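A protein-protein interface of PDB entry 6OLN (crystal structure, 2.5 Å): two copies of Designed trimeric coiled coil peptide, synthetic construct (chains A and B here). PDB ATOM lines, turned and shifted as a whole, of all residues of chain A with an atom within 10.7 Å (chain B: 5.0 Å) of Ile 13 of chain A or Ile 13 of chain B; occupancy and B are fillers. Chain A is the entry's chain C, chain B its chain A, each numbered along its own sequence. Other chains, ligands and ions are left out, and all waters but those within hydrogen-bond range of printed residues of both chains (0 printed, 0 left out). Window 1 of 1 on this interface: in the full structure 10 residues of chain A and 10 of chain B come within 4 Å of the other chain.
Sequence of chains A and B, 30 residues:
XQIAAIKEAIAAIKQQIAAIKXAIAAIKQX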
ATOM      1  N   ALA A   5      33.302  23.461   7.410  1.00  0.00           N
ATOM      2  CA  ALA A   5      33.130  22.190   6.711  1.00  0.00           C
ATOM      3  C   ALA A   5      32.036  22.275   5.652  1.00  0.00           C
ATOM      4  O   ALA A   5      32.163  21.692   4.569  1.00  0.00           O
ATOM      5  CB  ALA A   5      32.821  21.077   7.713  1.00  0.00           C
ATOM      6  N   ILE A   6      30.956  23.004   5.945  1.00  0.00           N
ATOM      7  CA  ILE A   6      29.842  23.117   5.004  1.00  0.00           C
ATOM      8  C   ILE A   6      30.269  23.869   3.751  1.00  0.00           C
ATOM      9  O   ILE A   6      29.941  23.472   2.625  1.00  0.00           O
ATOM     10  CB  ILE A   6      28.640  23.794   5.686  1.00  0.00           C
ATOM     11  CG1 ILE A   6      27.991  22.845   6.692  1.00  0.00           C
ATOM     12  CG2 ILE A   6      27.637  24.271   4.644  1.00  0.00           C
ATOM     13  CD1 ILE A   6      26.919  23.496   7.531  1.00  0.00           C
ATOM     14  N   LYS A   7      30.999  24.975   3.923  1.00  0.00           N
ATOM     15  CA  LYS A   7      31.446  25.759   2.776  1.00  0.00           C
ATOM     16  C   LYS A   7      32.522  25.023   1.981  1.00  0.00           C
ATOM     17  O   LYS A   7      32.578  25.136   0.750  1.00  0.00           O
ATOM     18  CB  LYS A   7      31.952  27.124   3.243  1.00  0.00           C
ATOM     19  CG  LYS A   7      30.839  28.054   3.716  1.00  0.00           C
ATOM     20  CD  LYS A   7      31.292  28.954   4.859  1.00  0.00           C
ATOM     21  CE  LYS A   7      32.108  30.143   4.376  1.00  0.00           C
ATOM     22  NZ  LYS A   7      32.286  31.162   5.457  1.00  0.00           N
ATOM     23  N   GLU A   8      33.383  24.264   2.668  1.00  0.00           N
ATOM     24  CA  GLU A   8      34.413  23.496   1.971  1.00  0.00           C
ATOM     25  C   GLU A   8      33.825  22.250   1.312  1.00  0.00           C
ATOM     26  O   GLU A   8      34.410  21.710   0.362  1.00  0.00           O
ATOM     27  CB  GLU A   8      35.542  23.134   2.946  1.00  0.00           C
ATOM     28  CG  GLU A   8      36.074  24.326   3.815  1.00  0.00           C
ATOM     29  CD  GLU A   8      37.255  23.909   4.704  1.00  0.00           C
ATOM     30  OE1 GLU A   8      37.941  22.993   4.244  1.00  0.00           O
ATOM     31  OE2 GLU A   8      37.488  24.438   5.823  1.00  0.00           O
ATOM     32  N   ALA A   9      32.665  21.794   1.785  1.00  0.00           N
ATOM     33  CA  ALA A   9      31.997  20.662   1.150  1.00  0.00           C
ATOM     34  C   ALA A   9      31.244  21.104  -0.097  1.00  0.00           C
ATOM     35  O   ALA A   9      31.164  20.360  -1.082  1.00  0.00           O
ATOM     36  CB  ALA A   9      31.049  19.990   2.145  1.00  0.00           C
ATOM     37  N   ILE A  10      30.701  22.323  -0.077  1.00  0.00           N
ATOM     38  CA  ILE A  10      29.993  22.853  -1.238  1.00  0.00           C
ATOM     39  C   ILE A  10      30.972  23.159  -2.364  1.00  0.00           C
ATOM     40  O   ILE A  10      30.683  22.907  -3.544  1.00  0.00           O
ATOM     41  CB  ILE A  10      29.179  24.094  -0.827  1.00  0.00           C
ATOM     42  CG1 ILE A  10      27.986  23.680   0.038  1.00  0.00           C
ATOM     43  CG2 ILE A  10      28.752  24.898  -2.048  1.00  0.00           C
ATOM     44  CD1 ILE A  10      27.300  24.848   0.712  1.00  0.00           C
ATOM     45  N   ALA A  11      32.146  23.692  -2.022  1.00  0.00           N
ATOM     46  CA  ALA A  11      33.164  23.965  -3.031  1.00  0.00           C
ATOM     47  C   ALA A  11      33.623  22.683  -3.714  1.00  0.00           C
ATOM     48  O   ALA A  11      33.897  22.678  -4.920  1.00  0.00           O
ATOM     49  CB  ALA A  11      34.349  24.690  -2.394  1.00  0.00           C
ATOM     50  N   ALA A  12      33.711  21.584  -2.962  1.00  0.00           N
ATOM     51  CA  ALA A  12      34.075  20.305  -3.564  1.00  0.00           C
ATOM     52  C   ALA A  12      32.949  19.767  -4.438  1.00  0.00           C
ATOM     53  O   ALA A  12      33.205  19.149  -5.480  1.00  0.00           O
ATOM     54  CB  ALA A  12      34.440  19.296  -2.476  1.00  0.00           C
ATOM     55  N   ILE A  13      31.697  19.984  -4.029  1.00  0.00           N
ATOM     56  CA  ILE A  13      30.559  19.525  -4.820  1.00  0.00           C
ATOM     57  C   ILE A  13      30.488  20.282  -6.140  1.00  0.00           C
ATOM     58  O   ILE A  13      30.177  19.701  -7.189  1.00  0.00           O
ATOM     59  CB  ILE A  13      29.259  19.663  -4.004  1.00  0.00           C
ATOM     60  CG1 ILE A  13      29.198  18.589  -2.916  1.00  0.00           C
ATOM     61  CG2 ILE A  13      28.030  19.592  -4.909  1.00  0.00           C
ATOM     62  CD1 ILE A  13      28.135  18.844  -1.870  1.00  0.00           C
ATOM     63  N   LYS A  14      30.785  21.583  -6.114  1.00  0.00           N
ATOM     64  CA  LYS A  14      30.793  22.366  -7.346  1.00  0.00           C
ATOM     65  C   LYS A  14      31.837  21.842  -8.324  1.00  0.00           C
ATOM     66  O   LYS A  14      31.601  21.812  -9.538  1.00  0.00           O
ATOM     67  CB  LYS A  14      31.043  23.841  -7.033  1.00  0.00           C
ATOM     68  CG  LYS A  14      29.880  24.545  -6.356  1.00  0.00           C
ATOM     69  CD  LYS A  14      30.222  25.995  -6.060  1.00  0.00           C
ATOM     70  CE  LYS A  14      29.044  26.715  -5.427  1.00  0.00           C
ATOM     71  NZ  LYS A  14      29.382  28.112  -5.037  1.00  0.00           N
ATOM     72  N   GLN A  15      32.998  21.422  -7.815  1.00  0.00           N
ATOM     73  CA  GLN A  15      34.019  20.850  -8.686  1.00  0.00           C
ATOM     74  C   GLN A  15      33.551  19.533  -9.287  1.00  0.00           C
ATOM     75  O   GLN A  15      33.861  19.224 -10.444  1.00  0.00           O
ATOM     76  CB  GLN A  15      35.324  20.660  -7.912  1.00  0.00           C
ATOM     77  CG  GLN A  15      35.962  21.964  -7.454  1.00  0.00           C
ATOM     78  CD  GLN A  15      36.415  22.830  -8.614  1.00  0.00           C
ATOM     79  OE1 GLN A  15      37.194  22.396  -9.462  1.00  0.00           O
ATOM     80  NE2 GLN A  15      35.926  24.064  -8.657  1.00  0.00           N
ATOM     81  N   GLN A  16      32.794  18.742  -8.520  1.00  0.00           N
ATOM     82  CA  GLN A  16      32.253  17.498  -9.053  1.00  0.00           C
ATOM     83  C   GLN A  16      31.197  17.765 -10.117  1.00  0.00           C
ATOM     84  O   GLN A  16      31.156  17.076 -11.143  1.00  0.00           O
ATOM     85  CB  GLN A  16      31.673  16.649  -7.923  1.00  0.00           C
ATOM     86  CG  GLN A  16      32.720  16.032  -7.018  1.00  0.00           C
ATOM     87  CD  GLN A  16      32.112  15.242  -5.877  1.00  0.00           C
ATOM     88  OE1 GLN A  16      31.179  15.699  -5.217  1.00  0.00           O
ATOM     89  NE2 GLN A  16      32.635  14.044  -5.643  1.00  0.00           N
ATOM     90  N   ILE A  17      30.337  18.760  -9.891  1.00  0.00           N
ATOM     91  CA  ILE A  17      29.296  19.092 -10.862  1.00  0.00           C
ATOM     92  C   ILE A  17      29.920  19.486 -12.194  1.00  0.00           C
ATOM     93  O   ILE A  17      29.488  19.031 -13.262  1.00  0.00           O
ATOM     94  CB  ILE A  17      28.392  20.213 -10.318  1.00  0.00           C
ATOM     95  CG1 ILE A  17      27.599  19.735  -9.098  1.00  0.00           C
ATOM     96  CG2 ILE A  17      27.444  20.694 -11.402  1.00  0.00           C
ATOM     97  CD1 ILE A  17      26.560  18.688  -9.416  1.00  0.00           C
ATOM     98  N   ALA A  18      30.943  20.343 -12.153  1.00  0.00           N
ATOM     99  CA  ALA A  18      31.577  20.794 -13.385  1.00  0.00           C
ATOM    100  C   ALA A  18      32.226  19.633 -14.125  1.00  0.00           C
ATOM    101  O   ALA A  18      32.143  19.548 -15.356  1.00  0.00           O
ATOM    102  CB  ALA A  18      32.605  21.884 -13.081  1.00  0.00           C
ATOM    103  N   ALA A  19      32.875  18.727 -13.393  1.00  0.00           N
ATOM    104  CA  ALA A  19      33.478  17.561 -14.029  1.00  0.00           C
ATOM    105  C   ALA A  19      32.422  16.614 -14.581  1.00  0.00           C
ATOM    106  O   ALA A  19      32.648  15.974 -15.614  1.00  0.00           O
ATOM    107  CB  ALA A  19      34.381  16.832 -13.040  1.00  0.00           C
ATOM    108  N   ILE A  20      31.268  16.514 -13.920  1.00  0.00           N
ATOM    109  CA  ILE A  20      30.187  15.668 -14.426  1.00  0.00           C
ATOM    110  C   ILE A  20      29.619  16.254 -15.713  1.00  0.00           C
ATOM    111  O   ILE A  20      29.361  15.533 -16.689  1.00  0.00           O
ATOM    112  CB  ILE A  20      29.095  15.497 -13.354  1.00  0.00           C
ATOM    113  CG1 ILE A  20      29.580  14.574 -12.233  1.00  0.00           C
ATOM    114  CG2 ILE A  20      27.819  14.959 -13.977  1.00  0.00           C
ATOM    115  CD1 ILE A  20      28.637  14.516 -11.053  1.00  0.00           C
ATOM    116  N   LYS A  21      29.419  17.567 -15.738  1.00  0.00           N
ATOM    117  CA  LYS A  21      28.922  18.258 -16.922  1.00  0.00           C
ATOM    118  C   LYS A  21      29.855  18.073 -18.118  1.00  0.00           C
ATOM    119  O   LYS A  21      29.396  17.921 -19.248  1.00  0.00           O
ATOM    120  CB  LYS A  21      28.734  19.751 -16.636  1.00  0.00           C
ATOM    121  CG  LYS A  21      27.535  20.083 -15.759  1.00  0.00           C
ATOM    122  CD  LYS A  21      27.507  21.573 -15.425  1.00  0.00           C
ATOM    123  CE  LYS A  21      26.177  21.964 -14.790  1.00  0.00           C
ATOM    124  NZ  LYS A  21      26.183  23.376 -14.313  1.00  0.00           N
ATOM    125  N   GLU B   8      21.304  29.240  -0.557  1.00  0.00           N
ATOM    126  CA  GLU B   8      21.151  29.518  -1.982  1.00  0.00           C
ATOM    127  C   GLU B   8      22.049  28.616  -2.817  1.00  0.00           C
ATOM    128  O   GLU B   8      21.639  28.136  -3.882  1.00  0.00           O
ATOM    129  CB  GLU B   8      21.452  30.991  -2.264  1.00  0.00           C
ATOM    130  CG  GLU B   8      21.159  31.436  -3.695  1.00  0.00           C
ATOM    131  CD  GLU B   8      22.287  31.128  -4.666  1.00  0.00           C
ATOM    132  OE1 GLU B   8      23.424  30.877  -4.211  1.00  0.00           O
ATOM    133  OE2 GLU B   8      22.036  31.138  -5.890  1.00  0.00           O
ATOM    134  N   ALA B   9      23.281  28.381  -2.358  1.00  0.00           N
ATOM    135  CA  ALA B   9      24.195  27.519  -3.100  1.00  0.00           C
ATOM    136  C   ALA B   9      23.647  26.104  -3.209  1.00  0.00           C
ATOM    137  O   ALA B   9      23.745  25.468  -4.267  1.00  0.00           O
ATOM    138  CB  ALA B   9      25.571  27.514  -2.433  1.00  0.00           C
ATOM    139  N   ILE B  10      23.057  25.596  -2.127  1.00  0.00           N
ATOM    140  CA  ILE B  10      22.462  24.264  -2.153  1.00  0.00           C
ATOM    141  C   ILE B  10      21.253  24.240  -3.081  1.00  0.00           C
ATOM    142  O   ILE B  10      21.068  23.293  -3.855  1.00  0.00           O
ATOM    143  CB  ILE B  10      22.105  23.825  -0.723  1.00  0.00           C
ATOM    144  CG1 ILE B  10      23.387  23.544   0.068  1.00  0.00           C
ATOM    145  CG2 ILE B  10      21.186  22.610  -0.740  1.00  0.00           C
ATOM    146  CD1 ILE B  10      23.171  23.407   1.558  1.00  0.00           C
ATOM    147  N   ALA B  11      20.424  25.286  -3.032  1.00  0.00           N
ATOM    148  CA  ALA B  11      19.271  25.358  -3.926  1.00  0.00           C
ATOM    149  C   ALA B  11      19.704  25.423  -5.384  1.00  0.00           C
ATOM    150  O   ALA B  11      19.065  24.817  -6.254  1.00  0.00           O
ATOM    151  CB  ALA B  11      18.403  26.564  -3.569  1.00  0.00           C
ATOM    152  N   ALA B  12      20.788  26.147  -5.675  1.00  0.00           N
ATOM    153  CA  ALA B  12      21.295  26.195  -7.042  1.00  0.00           C
ATOM    154  C   ALA B  12      21.913  24.863  -7.446  1.00  0.00           C
ATOM    155  O   ALA B  12      21.818  24.455  -8.611  1.00  0.00           O
ATOM    156  CB  ALA B  12      22.310  27.329  -7.188  1.00  0.00           C
ATOM    157  N   ILE B  13      22.545  24.166  -6.497  1.00  0.00           N
ATOM    158  CA  ILE B  13      23.129  22.858  -6.784  1.00  0.00           C
ATOM    159  C   ILE B  13      22.040  21.840  -7.100  1.00  0.00           C
ATOM    160  O   ILE B  13      22.195  20.996  -7.993  1.00  0.00           O
ATOM    161  CB  ILE B  13      24.007  22.398  -5.603  1.00  0.00           C
ATOM    162  CG1 ILE B  13      25.340  23.147  -5.597  1.00  0.00           C
ATOM    163  CG2 ILE B  13      24.244  20.895  -5.654  1.00  0.00           C
ATOM    164  CD1 ILE B  13      26.128  22.965  -4.318  1.00  0.00           C
ATOM    165  N   LYS B  14      20.921  21.900  -6.372  1.00  0.00           N
ATOM    166  CA  LYS B  14      19.846  20.936  -6.586  1.00  0.00           C
ATOM    167  C   LYS B  14      19.238  21.084  -7.975  1.00  0.00           C
ATOM    168  O   LYS B  14      18.832  20.093  -8.593  1.00  0.00           O
ATOM    169  CB  LYS B  14      18.775  21.094  -5.505  1.00  0.00           C
ATOM    170  CG  LYS B  14      19.268  20.730  -4.109  1.00  0.00           C
ATOM    171  CD  LYS B  14      18.433  21.372  -3.009  1.00  0.00           C
ATOM    172  CE  LYS B  14      17.272  20.488  -2.584  1.00  0.00           C
ATOM    173  NZ  LYS B  14      16.702  20.928  -1.278  1.00  0.00           N
ATOM    174  N   GLN B  15      19.175  22.316  -8.486  1.00  0.00           N
ATOM    175  CA  GLN B  15      18.660  22.526  -9.835  1.00  0.00           C
ATOM    176  C   GLN B  15      19.635  22.026 -10.891  1.00  0.00           C
ATOM    177  O   GLN B  15      19.209  21.576 -11.960  1.00  0.00           O
ATOM    178  CB  GLN B  15      18.345  24.005 -10.052  1.00  0.00           C
ATOM    179  CG  GLN B  15      17.148  24.494  -9.247  1.00  0.00           C
ATOM    180  CD  GLN B  15      16.930  25.986  -9.369  1.00  0.00           C
ATOM    181  OE1 GLN B  15      17.869  26.745  -9.609  1.00  0.00           O
ATOM    182  NE2 GLN B  15      15.686  26.414  -9.206  1.00  0.00           N
ATOM    183  N   GLN B  16      20.939  22.091 -10.614  1.00  0.00           N
ATOM    184  CA  GLN B  16      21.914  21.520 -11.537  1.00  0.00           C
ATOM    185  C   GLN B  16      21.872  19.998 -11.502  1.00  0.00           C
ATOM    186  O   GLN B  16      22.082  19.343 -12.527  1.00  0.00           O
ATOM    187  CB  GLN B  16      23.316  22.031 -11.202  1.00  0.00           C
ATOM    188  CG  GLN B  16      23.480  23.535 -11.371  1.00  0.00           C
ATOM    189  CD  GLN B  16      24.790  24.041 -10.800  1.00  0.00           C
ATOM    190  OE1 GLN B  16      25.768  23.301 -10.713  1.00  0.00           O
ATOM    191  NE2 GLN B  16      24.811  25.307 -10.399  1.00  0.00           N
ATOM    192  N   ILE B  17      21.596  19.423 -10.327  1.00  0.00           N
ATOM    193  CA  ILE B  17      21.466  17.972 -10.203  1.00  0.00           C
ATOM    194  C   ILE B  17      20.293  17.471 -11.034  1.00  0.00           C
ATOM    195  O   ILE B  17      20.389  16.450 -11.732  1.00  0.00           O
ATOM    196  CB  ILE B  17      21.310  17.578  -8.722  1.00  0.00           C
ATOM    197  CG1 ILE B  17      22.621  17.792  -7.959  1.00  0.00           C
ATOM    198  CG2 ILE B  17      20.830  16.137  -8.593  1.00  0.00           C
ATOM    199  CD1 ILE B  17      23.695  16.793  -8.300  1.00  0.00           C
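Of the 10 printed residues of chain B, 3 touch a printed residue of chain A. Of the 17 printed residues of chain A, 4 touch a printed residue of chain B. Among the printed residues, no Asp or Glu carboxylate lies within 4 Å of a Lys or Arg side-chain nitrogen of the other chain.
Among the printed residues, merely in contact across the chains: Ile 10 of chain A with Ile 13 of chain B (3.97 Å), Ile 13 of chain A with Ile 13 of chain B (3.9 Å), Ile 17 of chain A with Gln 16 of chain B (3.2 Å), Ile 17 of chain A with Ile 17 of chain B (3.6 Å) and Lys 21 of chain A with Gln 16 of chain B (3.6 Å).
No residue of chain A comes within 4 Å of Ala 9 of chain B. No residue of chain A comes within 4 Å of Ile 10 of chain B. No residue of chain A comes within 4 Å of Ala 11 of chain B. Gln 16 of chain B touches just these residues of chain A: Ile 17 and Lys 21. Ile 17 of chain B touches just one residue of chain A: Ile 17. Of the printed residues of chain B, Ile 17 of chain A touches Gln 16 and Ile 17. Of the printed residues of chain B, Ile 10 of chain A touches Ile 13. The nearest printed residue of chain B that does not touch Ile 13 of chain A is Ile 17 of chain B (6.2 Å).
Ile 10 of chain A touches Ile 13 of chain B, but with the chains exchanged Ile 13 of chain A does not touch Ile 10 of chain B (7.0 Å). Ile 13 of chain A touches its own counterpart, Ile 13 of chain B. Ile 17 of chain A touches Gln 16 of chain B, but with the chains exchanged Gln 16 of chain A does not touch Ile 17 of chain B (7.8 Å). Ile 17 of chain B touches its own counterpart, Ile 17 of chain A. 10 positions are printed for both chains. Of the 5 pairs that touch across the chains among the printed residues, 2 have their exchanged pair printed and touching as well.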
